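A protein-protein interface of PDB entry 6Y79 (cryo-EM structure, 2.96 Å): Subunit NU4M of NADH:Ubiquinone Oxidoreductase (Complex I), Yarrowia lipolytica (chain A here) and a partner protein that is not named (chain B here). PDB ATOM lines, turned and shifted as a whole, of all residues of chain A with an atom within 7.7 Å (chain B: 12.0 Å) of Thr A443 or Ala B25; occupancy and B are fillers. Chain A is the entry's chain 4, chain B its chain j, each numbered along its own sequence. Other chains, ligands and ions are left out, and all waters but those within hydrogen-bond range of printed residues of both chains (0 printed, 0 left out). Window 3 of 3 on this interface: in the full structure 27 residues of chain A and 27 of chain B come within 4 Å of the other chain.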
ATOM      1  N   ILE A 349       9.381 -13.438  -4.487  1.00  0.00           N
ATOM      2  CA  ILE A 349       9.204 -14.509  -5.458  1.00  0.00           C
ATOM      3  C   ILE A 349       9.968 -15.766  -5.052  1.00  0.00           C
ATOM      4  O   ILE A 349       9.722 -16.851  -5.583  1.00  0.00           O
ATOM      5  CB  ILE A 349       9.621 -13.969  -6.836  1.00  0.00           C
ATOM      6  CG1 ILE A 349       9.032 -12.573  -7.033  1.00  0.00           C
ATOM      7  CG2 ILE A 349       9.150 -14.863  -7.943  1.00  0.00           C
ATOM      8  CD1 ILE A 349       9.268 -11.984  -8.394  1.00  0.00           C
ATOM      9  N   ASP A 352       8.398 -16.760  -0.677  1.00  0.00           N
ATOM     10  CA  ASP A 352       7.015 -17.215  -0.613  1.00  0.00           C
ATOM     11  C   ASP A 352       6.846 -18.609  -1.186  1.00  0.00           C
ATOM     12  O   ASP A 352       5.927 -19.324  -0.780  1.00  0.00           O
ATOM     13  CB  ASP A 352       6.088 -16.271  -1.373  1.00  0.00           C
ATOM     14  CG  ASP A 352       5.714 -15.049  -0.575  1.00  0.00           C
ATOM     15  OD1 ASP A 352       5.410 -15.202   0.624  1.00  0.00           O
ATOM     16  OD2 ASP A 352       5.715 -13.937  -1.143  1.00  0.00           O
ATOM     17  N   ARG A 353       7.704 -19.007  -2.117  1.00  0.00           N
ATOM     18  CA  ARG A 353       7.558 -20.277  -2.807  1.00  0.00           C
ATOM     19  C   ARG A 353       8.263 -21.416  -2.087  1.00  0.00           C
ATOM     20  O   ARG A 353       7.750 -22.535  -2.079  1.00  0.00           O
ATOM     21  CB  ARG A 353       8.097 -20.174  -4.239  1.00  0.00           C
ATOM     22  CG  ARG A 353       7.127 -19.698  -5.322  1.00  0.00           C
ATOM     23  CD  ARG A 353       6.851 -18.216  -5.205  1.00  0.00           C
ATOM     24  NE  ARG A 353       6.282 -17.594  -6.393  1.00  0.00           N
ATOM     25  CZ  ARG A 353       5.758 -16.372  -6.390  1.00  0.00           C
ATOM     26  NH1 ARG A 353       5.251 -15.857  -7.497  1.00  0.00           N
ATOM     27  NH2 ARG A 353       5.739 -15.659  -5.270  1.00  0.00           N
ATOM     28  N   TYR A 354       9.416 -21.166  -1.462  1.00  0.00           N
ATOM     29  CA  TYR A 354      10.220 -22.244  -0.906  1.00  0.00           C
ATOM     30  C   TYR A 354      10.574 -22.094   0.562  1.00  0.00           C
ATOM     31  O   TYR A 354      11.012 -23.079   1.161  1.00  0.00           O
ATOM     32  CB  TYR A 354      11.515 -22.408  -1.713  1.00  0.00           C
ATOM     33  CG  TYR A 354      11.223 -22.725  -3.150  1.00  0.00           C
ATOM     34  CD1 TYR A 354      10.836 -23.999  -3.526  1.00  0.00           C
ATOM     35  CD2 TYR A 354      11.294 -21.747  -4.124  1.00  0.00           C
ATOM     36  CE1 TYR A 354      10.543 -24.292  -4.831  1.00  0.00           C
ATOM     37  CE2 TYR A 354      10.999 -22.032  -5.431  1.00  0.00           C
ATOM     38  CZ  TYR A 354      10.625 -23.307  -5.776  1.00  0.00           C
ATOM     39  OH  TYR A 354      10.336 -23.598  -7.083  1.00  0.00           O
ATOM     40  N   HIS A 355      10.423 -20.907   1.147  1.00  0.00           N
ATOM     41  CA  HIS A 355      10.564 -20.614   2.574  1.00  0.00           C
ATOM     42  C   HIS A 355      11.952 -20.911   3.128  1.00  0.00           C
ATOM     43  O   HIS A 355      12.118 -21.010   4.347  1.00  0.00           O
ATOM     44  CB  HIS A 355       9.505 -21.339   3.410  1.00  0.00           C
ATOM     45  CG  HIS A 355       8.105 -20.931   3.086  1.00  0.00           C
ATOM     46  ND1 HIS A 355       7.580 -19.715   3.462  1.00  0.00           N
ATOM     47  CD2 HIS A 355       7.121 -21.575   2.417  1.00  0.00           C
ATOM     48  CE1 HIS A 355       6.332 -19.627   3.038  1.00  0.00           C
ATOM     49  NE2 HIS A 355       6.029 -20.741   2.400  1.00  0.00           N
ATOM     50  N   TYR A 368      12.324 -23.572 -15.555  1.00  0.00           N
ATOM     51  CA  TYR A 368      10.945 -23.551 -15.105  1.00  0.00           C
ATOM     52  C   TYR A 368      10.393 -22.148 -14.961  1.00  0.00           C
ATOM     53  O   TYR A 368       9.175 -21.973 -15.010  1.00  0.00           O
ATOM     54  CB  TYR A 368      10.798 -24.260 -13.752  1.00  0.00           C
ATOM     55  CG  TYR A 368      11.038 -25.748 -13.773  1.00  0.00           C
ATOM     56  CD1 TYR A 368      10.852 -26.494 -14.931  1.00  0.00           C
ATOM     57  CD2 TYR A 368      11.462 -26.407 -12.629  1.00  0.00           C
ATOM     58  CE1 TYR A 368      11.080 -27.851 -14.943  1.00  0.00           C
ATOM     59  CE2 TYR A 368      11.694 -27.759 -12.631  1.00  0.00           C
ATOM     60  CZ  TYR A 368      11.502 -28.476 -13.790  1.00  0.00           C
ATOM     61  OH  TYR A 368      11.731 -29.827 -13.787  1.00  0.00           O
ATOM     62  N   MET A 369      11.255 -21.154 -14.760  1.00  0.00           N
ATOM     63  CA  MET A 369      10.854 -19.764 -14.560  1.00  0.00           C
ATOM     64  C   MET A 369      11.691 -18.893 -15.477  1.00  0.00           C
ATOM     65  O   MET A 369      12.697 -18.320 -15.050  1.00  0.00           O
ATOM     66  CB  MET A 369      11.052 -19.337 -13.111  1.00  0.00           C
ATOM     67  CG  MET A 369      10.231 -20.091 -12.116  1.00  0.00           C
ATOM     68  SD  MET A 369      10.802 -19.700 -10.472  1.00  0.00           S
ATOM     69  CE  MET A 369       9.476 -20.374  -9.515  1.00  0.00           C
ATOM     70  N   ILE A 438      17.399 -30.253  -7.674  1.00  0.00           N
ATOM     71  CA  ILE A 438      16.709 -31.447  -7.220  1.00  0.00           C
ATOM     72  C   ILE A 438      16.012 -31.203  -5.896  1.00  0.00           C
ATOM     73  O   ILE A 438      15.150 -31.991  -5.498  1.00  0.00           O
ATOM     74  CB  ILE A 438      17.695 -32.619  -7.124  1.00  0.00           C
ATOM     75  CG1 ILE A 438      18.812 -32.289  -6.147  1.00  0.00           C
ATOM     76  CG2 ILE A 438      18.272 -32.926  -8.485  1.00  0.00           C
ATOM     77  CD1 ILE A 438      19.751 -33.417  -5.936  1.00  0.00           C
ATOM     78  N   TYR A 439      16.361 -30.121  -5.205  1.00  0.00           N
ATOM     79  CA  TYR A 439      15.690 -29.762  -3.965  1.00  0.00           C
ATOM     80  C   TYR A 439      14.395 -29.014  -4.231  1.00  0.00           C
ATOM     81  O   TYR A 439      13.386 -29.268  -3.572  1.00  0.00           O
ATOM     82  CB  TYR A 439      16.619 -28.921  -3.103  1.00  0.00           C
ATOM     83  CG  TYR A 439      17.846 -29.664  -2.666  1.00  0.00           C
ATOM     84  CD1 TYR A 439      17.764 -30.637  -1.687  1.00  0.00           C
ATOM     85  CD2 TYR A 439      19.085 -29.395  -3.230  1.00  0.00           C
ATOM     86  CE1 TYR A 439      18.873 -31.324  -1.280  1.00  0.00           C
ATOM     87  CE2 TYR A 439      20.208 -30.077  -2.825  1.00  0.00           C
ATOM     88  CZ  TYR A 439      20.093 -31.040  -1.851  1.00  0.00           C
ATOM     89  OH  TYR A 439      21.202 -31.734  -1.430  1.00  0.00           O
ATOM     90  N   MET A 440      14.406 -28.094  -5.185  1.00  0.00           N
ATOM     91  CA  MET A 440      13.214 -27.326  -5.513  1.00  0.00           C
ATOM     92  C   MET A 440      12.274 -28.165  -6.364  1.00  0.00           C
ATOM     93  O   MET A 440      12.660 -28.654  -7.429  1.00  0.00           O
ATOM     94  CB  MET A 440      13.575 -26.052  -6.269  1.00  0.00           C
ATOM     95  CG  MET A 440      14.515 -25.103  -5.571  1.00  0.00           C
ATOM     96  SD  MET A 440      15.291 -24.083  -6.834  1.00  0.00           S
ATOM     97  CE  MET A 440      13.944 -22.999  -7.288  1.00  0.00           C
ATOM     98  N   HIS A 441      11.043 -28.321  -5.904  1.00  0.00           N
ATOM     99  CA  HIS A 441       9.984 -28.751  -6.795  1.00  0.00           C
ATOM    100  C   HIS A 441       9.424 -27.540  -7.523  1.00  0.00           C
ATOM    101  O   HIS A 441       9.461 -26.417  -7.020  1.00  0.00           O
ATOM    102  CB  HIS A 441       8.880 -29.472  -6.028  1.00  0.00           C
ATOM    103  CG  HIS A 441       7.892 -30.164  -6.909  1.00  0.00           C
ATOM    104  ND1 HIS A 441       6.770 -29.536  -7.400  1.00  0.00           N
ATOM    105  CD2 HIS A 441       7.866 -31.423  -7.406  1.00  0.00           C
ATOM    106  CE1 HIS A 441       6.089 -30.379  -8.153  1.00  0.00           C
ATOM    107  NE2 HIS A 441       6.734 -31.530  -8.176  1.00  0.00           N
ATOM    108  N   ARG A 442       8.923 -27.779  -8.726  1.00  0.00           N
ATOM    109  CA  ARG A 442       8.473 -26.716  -9.606  1.00  0.00           C
ATOM    110  C   ARG A 442       7.252 -25.998  -9.049  1.00  0.00           C
ATOM    111  O   ARG A 442       6.285 -26.632  -8.631  1.00  0.00           O
ATOM    112  CB  ARG A 442       8.129 -27.315 -10.955  1.00  0.00           C
ATOM    113  CG  ARG A 442       7.522 -26.361 -11.892  1.00  0.00           C
ATOM    114  CD  ARG A 442       6.914 -27.066 -13.027  1.00  0.00           C
ATOM    115  NE  ARG A 442       6.880 -26.137 -14.141  1.00  0.00           N
ATOM    116  CZ  ARG A 442       6.690 -26.487 -15.402  1.00  0.00           C
ATOM    117  NH1 ARG A 442       6.495 -27.757 -15.717  1.00  0.00           N
ATOM    118  NH2 ARG A 442       6.710 -25.565 -16.337  1.00  0.00           N
ATOM    119  N   THR A 443       7.286 -24.669  -9.057  1.00  0.00           N
ATOM    120  CA  THR A 443       6.159 -23.864  -8.613  1.00  0.00           C
ATOM    121  C   THR A 443       5.693 -22.944  -9.736  1.00  0.00           C
ATOM    122  O   THR A 443       6.109 -23.073 -10.888  1.00  0.00           O
ATOM    123  CB  THR A 443       6.511 -23.058  -7.365  1.00  0.00           C
ATOM    124  OG1 THR A 443       7.691 -22.298  -7.608  1.00  0.00           O
ATOM    125  CG2 THR A 443       6.755 -23.967  -6.204  1.00  0.00           C
ATOM    126  N   ASN A 444       4.791 -22.034  -9.387  1.00  0.00           N
ATOM    127  CA  ASN A 444       4.235 -21.086 -10.334  1.00  0.00           C
ATOM    128  C   ASN A 444       5.307 -20.137 -10.840  1.00  0.00           C
ATOM    129  O   ASN A 444       6.284 -19.836 -10.157  1.00  0.00           O
ATOM    130  CB  ASN A 444       3.128 -20.262  -9.686  1.00  0.00           C
ATOM    131  CG  ASN A 444       1.923 -21.082  -9.335  1.00  0.00           C
ATOM    132  OD1 ASN A 444       1.263 -21.637 -10.206  1.00  0.00           O
ATOM    133  ND2 ASN A 444       1.622 -21.166  -8.047  1.00  0.00           N
ATOM    134  N   ASP A 445       5.102 -19.638 -12.050  1.00  0.00           N
ATOM    135  CA  ASP A 445       5.917 -18.529 -12.503  1.00  0.00           C
ATOM    136  C   ASP A 445       5.427 -17.236 -11.861  1.00  0.00           C
ATOM    137  O   ASP A 445       4.458 -17.216 -11.097  1.00  0.00           O
ATOM    138  CB  ASP A 445       5.890 -18.421 -14.023  1.00  0.00           C
ATOM    139  CG  ASP A 445       7.213 -17.958 -14.593  1.00  0.00           C
ATOM    140  OD1 ASP A 445       8.126 -17.643 -13.807  1.00  0.00           O
ATOM    141  OD2 ASP A 445       7.336 -17.904 -15.832  1.00  0.00           O
ATOM    142  N   VAL A 446       6.127 -16.146 -12.179  1.00  0.00           N
ATOM    143  CA  VAL A 446       5.893 -14.878 -11.506  1.00  0.00           C
ATOM    144  C   VAL A 446       4.531 -14.329 -11.881  1.00  0.00           C
ATOM    145  O   VAL A 446       4.052 -14.492 -13.009  1.00  0.00           O
ATOM    146  CB  VAL A 446       7.035 -13.900 -11.812  1.00  0.00           C
ATOM    147  CG1 VAL A 446       8.279 -14.528 -11.419  1.00  0.00           C
ATOM    148  CG2 VAL A 446       7.143 -13.620 -13.285  1.00  0.00           C
ATOM    149  N   TRP B  20      -4.523 -21.380   4.485  1.00  0.00           N
ATOM    150  CA  TRP B  20      -4.318 -22.549   3.650  1.00  0.00           C
ATOM    151  C   TRP B  20      -2.955 -23.138   3.958  1.00  0.00           C
ATOM    152  O   TRP B  20      -1.971 -22.406   4.078  1.00  0.00           O
ATOM    153  CB  TRP B  20      -4.404 -22.142   2.185  1.00  0.00           C
ATOM    154  CG  TRP B  20      -4.319 -23.214   1.157  1.00  0.00           C
ATOM    155  CD1 TRP B  20      -5.197 -24.229   0.951  1.00  0.00           C
ATOM    156  CD2 TRP B  20      -3.321 -23.332   0.142  1.00  0.00           C
ATOM    157  NE1 TRP B  20      -4.797 -24.988  -0.118  1.00  0.00           N
ATOM    158  CE2 TRP B  20      -3.645 -24.457  -0.632  1.00  0.00           C
ATOM    159  CE3 TRP B  20      -2.177 -22.601  -0.179  1.00  0.00           C
ATOM    160  CZ2 TRP B  20      -2.867 -24.868  -1.706  1.00  0.00           C
ATOM    161  CZ3 TRP B  20      -1.412 -23.010  -1.238  1.00  0.00           C
ATOM    162  CH2 TRP B  20      -1.756 -24.129  -1.992  1.00  0.00           C
ATOM    163  N   ASP B  21      -2.894 -24.455   4.105  1.00  0.00           N
ATOM    164  CA  ASP B  21      -1.599 -25.107   4.260  1.00  0.00           C
ATOM    165  C   ASP B  21      -1.035 -25.363   2.874  1.00  0.00           C
ATOM    166  O   ASP B  21      -1.503 -26.247   2.152  1.00  0.00           O
ATOM    167  CB  ASP B  21      -1.705 -26.397   5.057  1.00  0.00           C
ATOM    168  CG  ASP B  21      -0.378 -26.784   5.677  1.00  0.00           C
ATOM    169  OD1 ASP B  21       0.269 -25.887   6.255  1.00  0.00           O
ATOM    170  OD2 ASP B  21       0.031 -27.958   5.575  1.00  0.00           O
ATOM    171  N   ALA B  22      -0.038 -24.574   2.499  1.00  0.00           N
ATOM    172  CA  ALA B  22       0.622 -24.741   1.214  1.00  0.00           C
ATOM    173  C   ALA B  22       1.406 -26.043   1.219  1.00  0.00           C
ATOM    174  O   ALA B  22       2.131 -26.308   2.184  1.00  0.00           O
ATOM    175  CB  ALA B  22       1.545 -23.565   0.931  1.00  0.00           C
ATOM    176  N   PRO B  23       1.255 -26.899   0.212  1.00  0.00           N
ATOM    177  CA  PRO B  23       2.053 -28.125   0.161  1.00  0.00           C
ATOM    178  C   PRO B  23       3.526 -27.822  -0.062  1.00  0.00           C
ATOM    179  O   PRO B  23       3.895 -26.774  -0.597  1.00  0.00           O
ATOM    180  CB  PRO B  23       1.454 -28.891  -1.021  1.00  0.00           C
ATOM    181  CG  PRO B  23       0.749 -27.861  -1.829  1.00  0.00           C
ATOM    182  CD  PRO B  23       0.252 -26.850  -0.861  1.00  0.00           C
ATOM    183  N   HIS B  24       4.367 -28.762   0.365  1.00  0.00           N
ATOM    184  CA  HIS B  24       5.802 -28.523   0.481  1.00  0.00           C
ATOM    185  C   HIS B  24       6.447 -28.488  -0.894  1.00  0.00           C
ATOM    186  O   HIS B  24       6.543 -29.512  -1.575  1.00  0.00           O
ATOM    187  CB  HIS B  24       6.443 -29.596   1.352  1.00  0.00           C
ATOM    188  CG  HIS B  24       5.960 -29.579   2.765  1.00  0.00           C
ATOM    189  ND1 HIS B  24       4.855 -30.288   3.183  1.00  0.00           N
ATOM    190  CD2 HIS B  24       6.419 -28.922   3.856  1.00  0.00           C
ATOM    191  CE1 HIS B  24       4.659 -30.077   4.471  1.00  0.00           C
ATOM    192  NE2 HIS B  24       5.595 -29.251   4.904  1.00  0.00           N
ATOM    193  N   ALA B  25       6.893 -27.304  -1.298  1.00  0.00           N
ATOM    194  CA  ALA B  25       7.564 -27.115  -2.571  1.00  0.00           C
ATOM    195  C   ALA B  25       9.043 -27.433  -2.509  1.00  0.00           C
ATOM    196  O   ALA B  25       9.702 -27.441  -3.550  1.00  0.00           O
ATOM    197  CB  ALA B  25       7.389 -25.681  -3.041  1.00  0.00           C
ATOM    198  N   LEU B  26       9.582 -27.693  -1.327  1.00  0.00           N
ATOM    199  CA  LEU B  26      11.017 -27.842  -1.181  1.00  0.00           C
ATOM    200  C   LEU B  26      11.326 -28.977  -0.228  1.00  0.00           C
ATOM    201  O   LEU B  26      10.843 -28.988   0.906  1.00  0.00           O
ATOM    202  CB  LEU B  26      11.655 -26.559  -0.663  1.00  0.00           C
ATOM    203  CG  LEU B  26      13.156 -26.699  -0.432  1.00  0.00           C
ATOM    204  CD1 LEU B  26      13.930 -26.336  -1.681  1.00  0.00           C
ATOM    205  CD2 LEU B  26      13.589 -25.872   0.739  1.00  0.00           C
ATOM    206  N   HIS B  27      12.137 -29.923  -0.688  1.00  0.00           N
ATOM    207  CA  HIS B  27      12.651 -30.980   0.169  1.00  0.00           C
ATOM    208  C   HIS B  27      13.826 -30.428   0.954  1.00  0.00           C
ATOM    209  O   HIS B  27      14.824 -30.014   0.366  1.00  0.00           O
ATOM    210  CB  HIS B  27      13.071 -32.185  -0.663  1.00  0.00           C
ATOM    211  CG  HIS B  27      12.038 -32.621  -1.648  1.00  0.00           C
ATOM    212  ND1 HIS B  27      11.923 -32.064  -2.902  1.00  0.00           N
ATOM    213  CD2 HIS B  27      11.056 -33.546  -1.553  1.00  0.00           C
ATOM    214  CE1 HIS B  27      10.920 -32.634  -3.542  1.00  0.00           C
ATOM    215  NE2 HIS B  27      10.377 -33.537  -2.746  1.00  0.00           N
ATOM    216  N   ASN B  28      13.693 -30.406   2.275  1.00  0.00           N
ATOM    217  CA  ASN B  28      14.749 -29.954   3.160  1.00  0.00           C
ATOM    218  C   ASN B  28      15.961 -30.855   3.016  1.00  0.00           C
ATOM    219  O   ASN B  28      15.856 -32.061   2.760  1.00  0.00           O
ATOM    220  CB  ASN B  28      14.314 -29.977   4.611  1.00  0.00           C
ATOM    221  CG  ASN B  28      13.110 -29.091   4.876  1.00  0.00           C
ATOM    222  OD1 ASN B  28      12.008 -29.586   5.122  1.00  0.00           O
ATOM    223  ND2 ASN B  28      13.320 -27.782   4.884  1.00  0.00           N
ATOM    224  N   ASP B  29      17.127 -30.238   3.122  1.00  0.00           N
ATOM    225  CA  ASP B  29      18.390 -30.954   3.270  1.00  0.00           C
ATOM    226  C   ASP B  29      18.923 -30.729   4.664  1.00  0.00           C
ATOM    227  O   ASP B  29      19.158 -29.591   5.058  1.00  0.00           O
ATOM    228  CB  ASP B  29      19.400 -30.504   2.220  1.00  0.00           C
ATOM    229  CG  ASP B  29      20.688 -31.346   2.173  1.00  0.00           C
ATOM    230  OD1 ASP B  29      21.157 -31.949   3.133  1.00  0.00           O
ATOM    231  OD2 ASP B  29      21.115 -31.547   1.007  1.00  0.00           O
ATOM    232  N   ASP B  33      21.006 -27.430   5.822  1.00  0.00           N
ATOM    233  CA  ASP B  33      20.418 -26.662   6.917  1.00  0.00           C
ATOM    234  C   ASP B  33      21.363 -26.574   8.104  1.00  0.00           C
ATOM    235  O   ASP B  33      21.486 -25.512   8.720  1.00  0.00           O
ATOM    236  CB  ASP B  33      19.083 -27.267   7.349  1.00  0.00           C
ATOM    237  CG  ASP B  33      17.983 -27.047   6.333  1.00  0.00           C
ATOM    238  OD1 ASP B  33      18.124 -26.138   5.492  1.00  0.00           O
ATOM    239  OD2 ASP B  33      16.983 -27.793   6.364  1.00  0.00           O
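Among the printed residues, merely in contact across the chains: Arg A353 with Ala B25 (3.3 Å), Tyr A354 with Ala B25 (3.5 Å), Tyr A354 with Leu B26 (3.8 Å), Tyr A439 with Leu B26 (3.5 Å), Met A440 with Ala B25 (3.9 Å), Met A440 with Leu B26 (3.9 Å) and Thr A443 with Ala B25 (3.7 Å).
The side-chain hydroxyl (OH) of Tyr A354 sits at hydrogen-bond distance from the backbone carbonyl oxygen (O) of His A441 (3.0 Å). The side-chain hydroxyl of Tyr A354 is in hydrogen-bond range of the side-chain hydroxyl of Thr A443, at 3.0 Å.
Printed residues of chain B that touch a printed residue of chain A: Ala B25, Leu B26, His B27 and Asp B29. Hydrophobic or aromatic side chains of chain B that line the printed part of chain A: Ala B25, Leu B26 and His B27. Of the 16 printed residues of chain A, 6 touch a printed residue of chain B. Hydrophobic or aromatic side chains of chain A that line the printed part of chain B: Tyr A354, Tyr A439 and His A441. Among the printed residues, 10 pairs touch across the chains. Among the printed residues, no Asp or Glu carboxylate lies within 4 Å of a Lys or Arg side-chain nitrogen of the other chain.
N of His A441 is in hydrogen-bond range of O of Ala B25 (2.8 Å). The backbone carbonyl oxygen (O) of Tyr A439 is in hydrogen-bond range of the backbone NH (N) of His B27. OD2 of Asp B29 is in hydrogen-bond range of OH of Tyr A439 (2.4 Å).
Tyr A354 touches just these residues of chain B: Ala B25 (3.5 Å) and Leu B26 (3.8 Å). Printed residues of chain B within 4 Å of Tyr A439: Leu B26 (3.5 Å), His B27 (3.2 Å) and Asp B29 (2.4 Å). Of chain B, only Ala B25 (3.9 Å) and Leu B26 (3.9 Å) come within 4 Å of Met A440. His A441 touches just one residue of chain B: Ala B25. No residue of chain B comes within 4 Å of Arg A442. No residue of chain B comes within 4 Å of Asn A444. No residue of chain B comes within 4 Å of Asp A445. Of the printed residues of chain A, Ala B25 touches Arg A353 (3.3 Å), Tyr A354 (3.5 Å), Met A440 (3.9 Å), His A441 (2.8 Å) and Thr A443 (3.7 Å). Printed residues of chain A within 4 Å of Leu B26: Tyr A354 (3.8 Å), Tyr A439 (3.5 Å) and Met A440 (3.9 Å). Of the printed residues of chain A, His B27 touches Tyr A439 (3.2 Å). Of the printed residues of chain A, Asp B29 touches Tyr A439 (2.4 Å). The nearest residue of chain B that does not touch Thr A443 is Leu B26 (6.8 Å).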
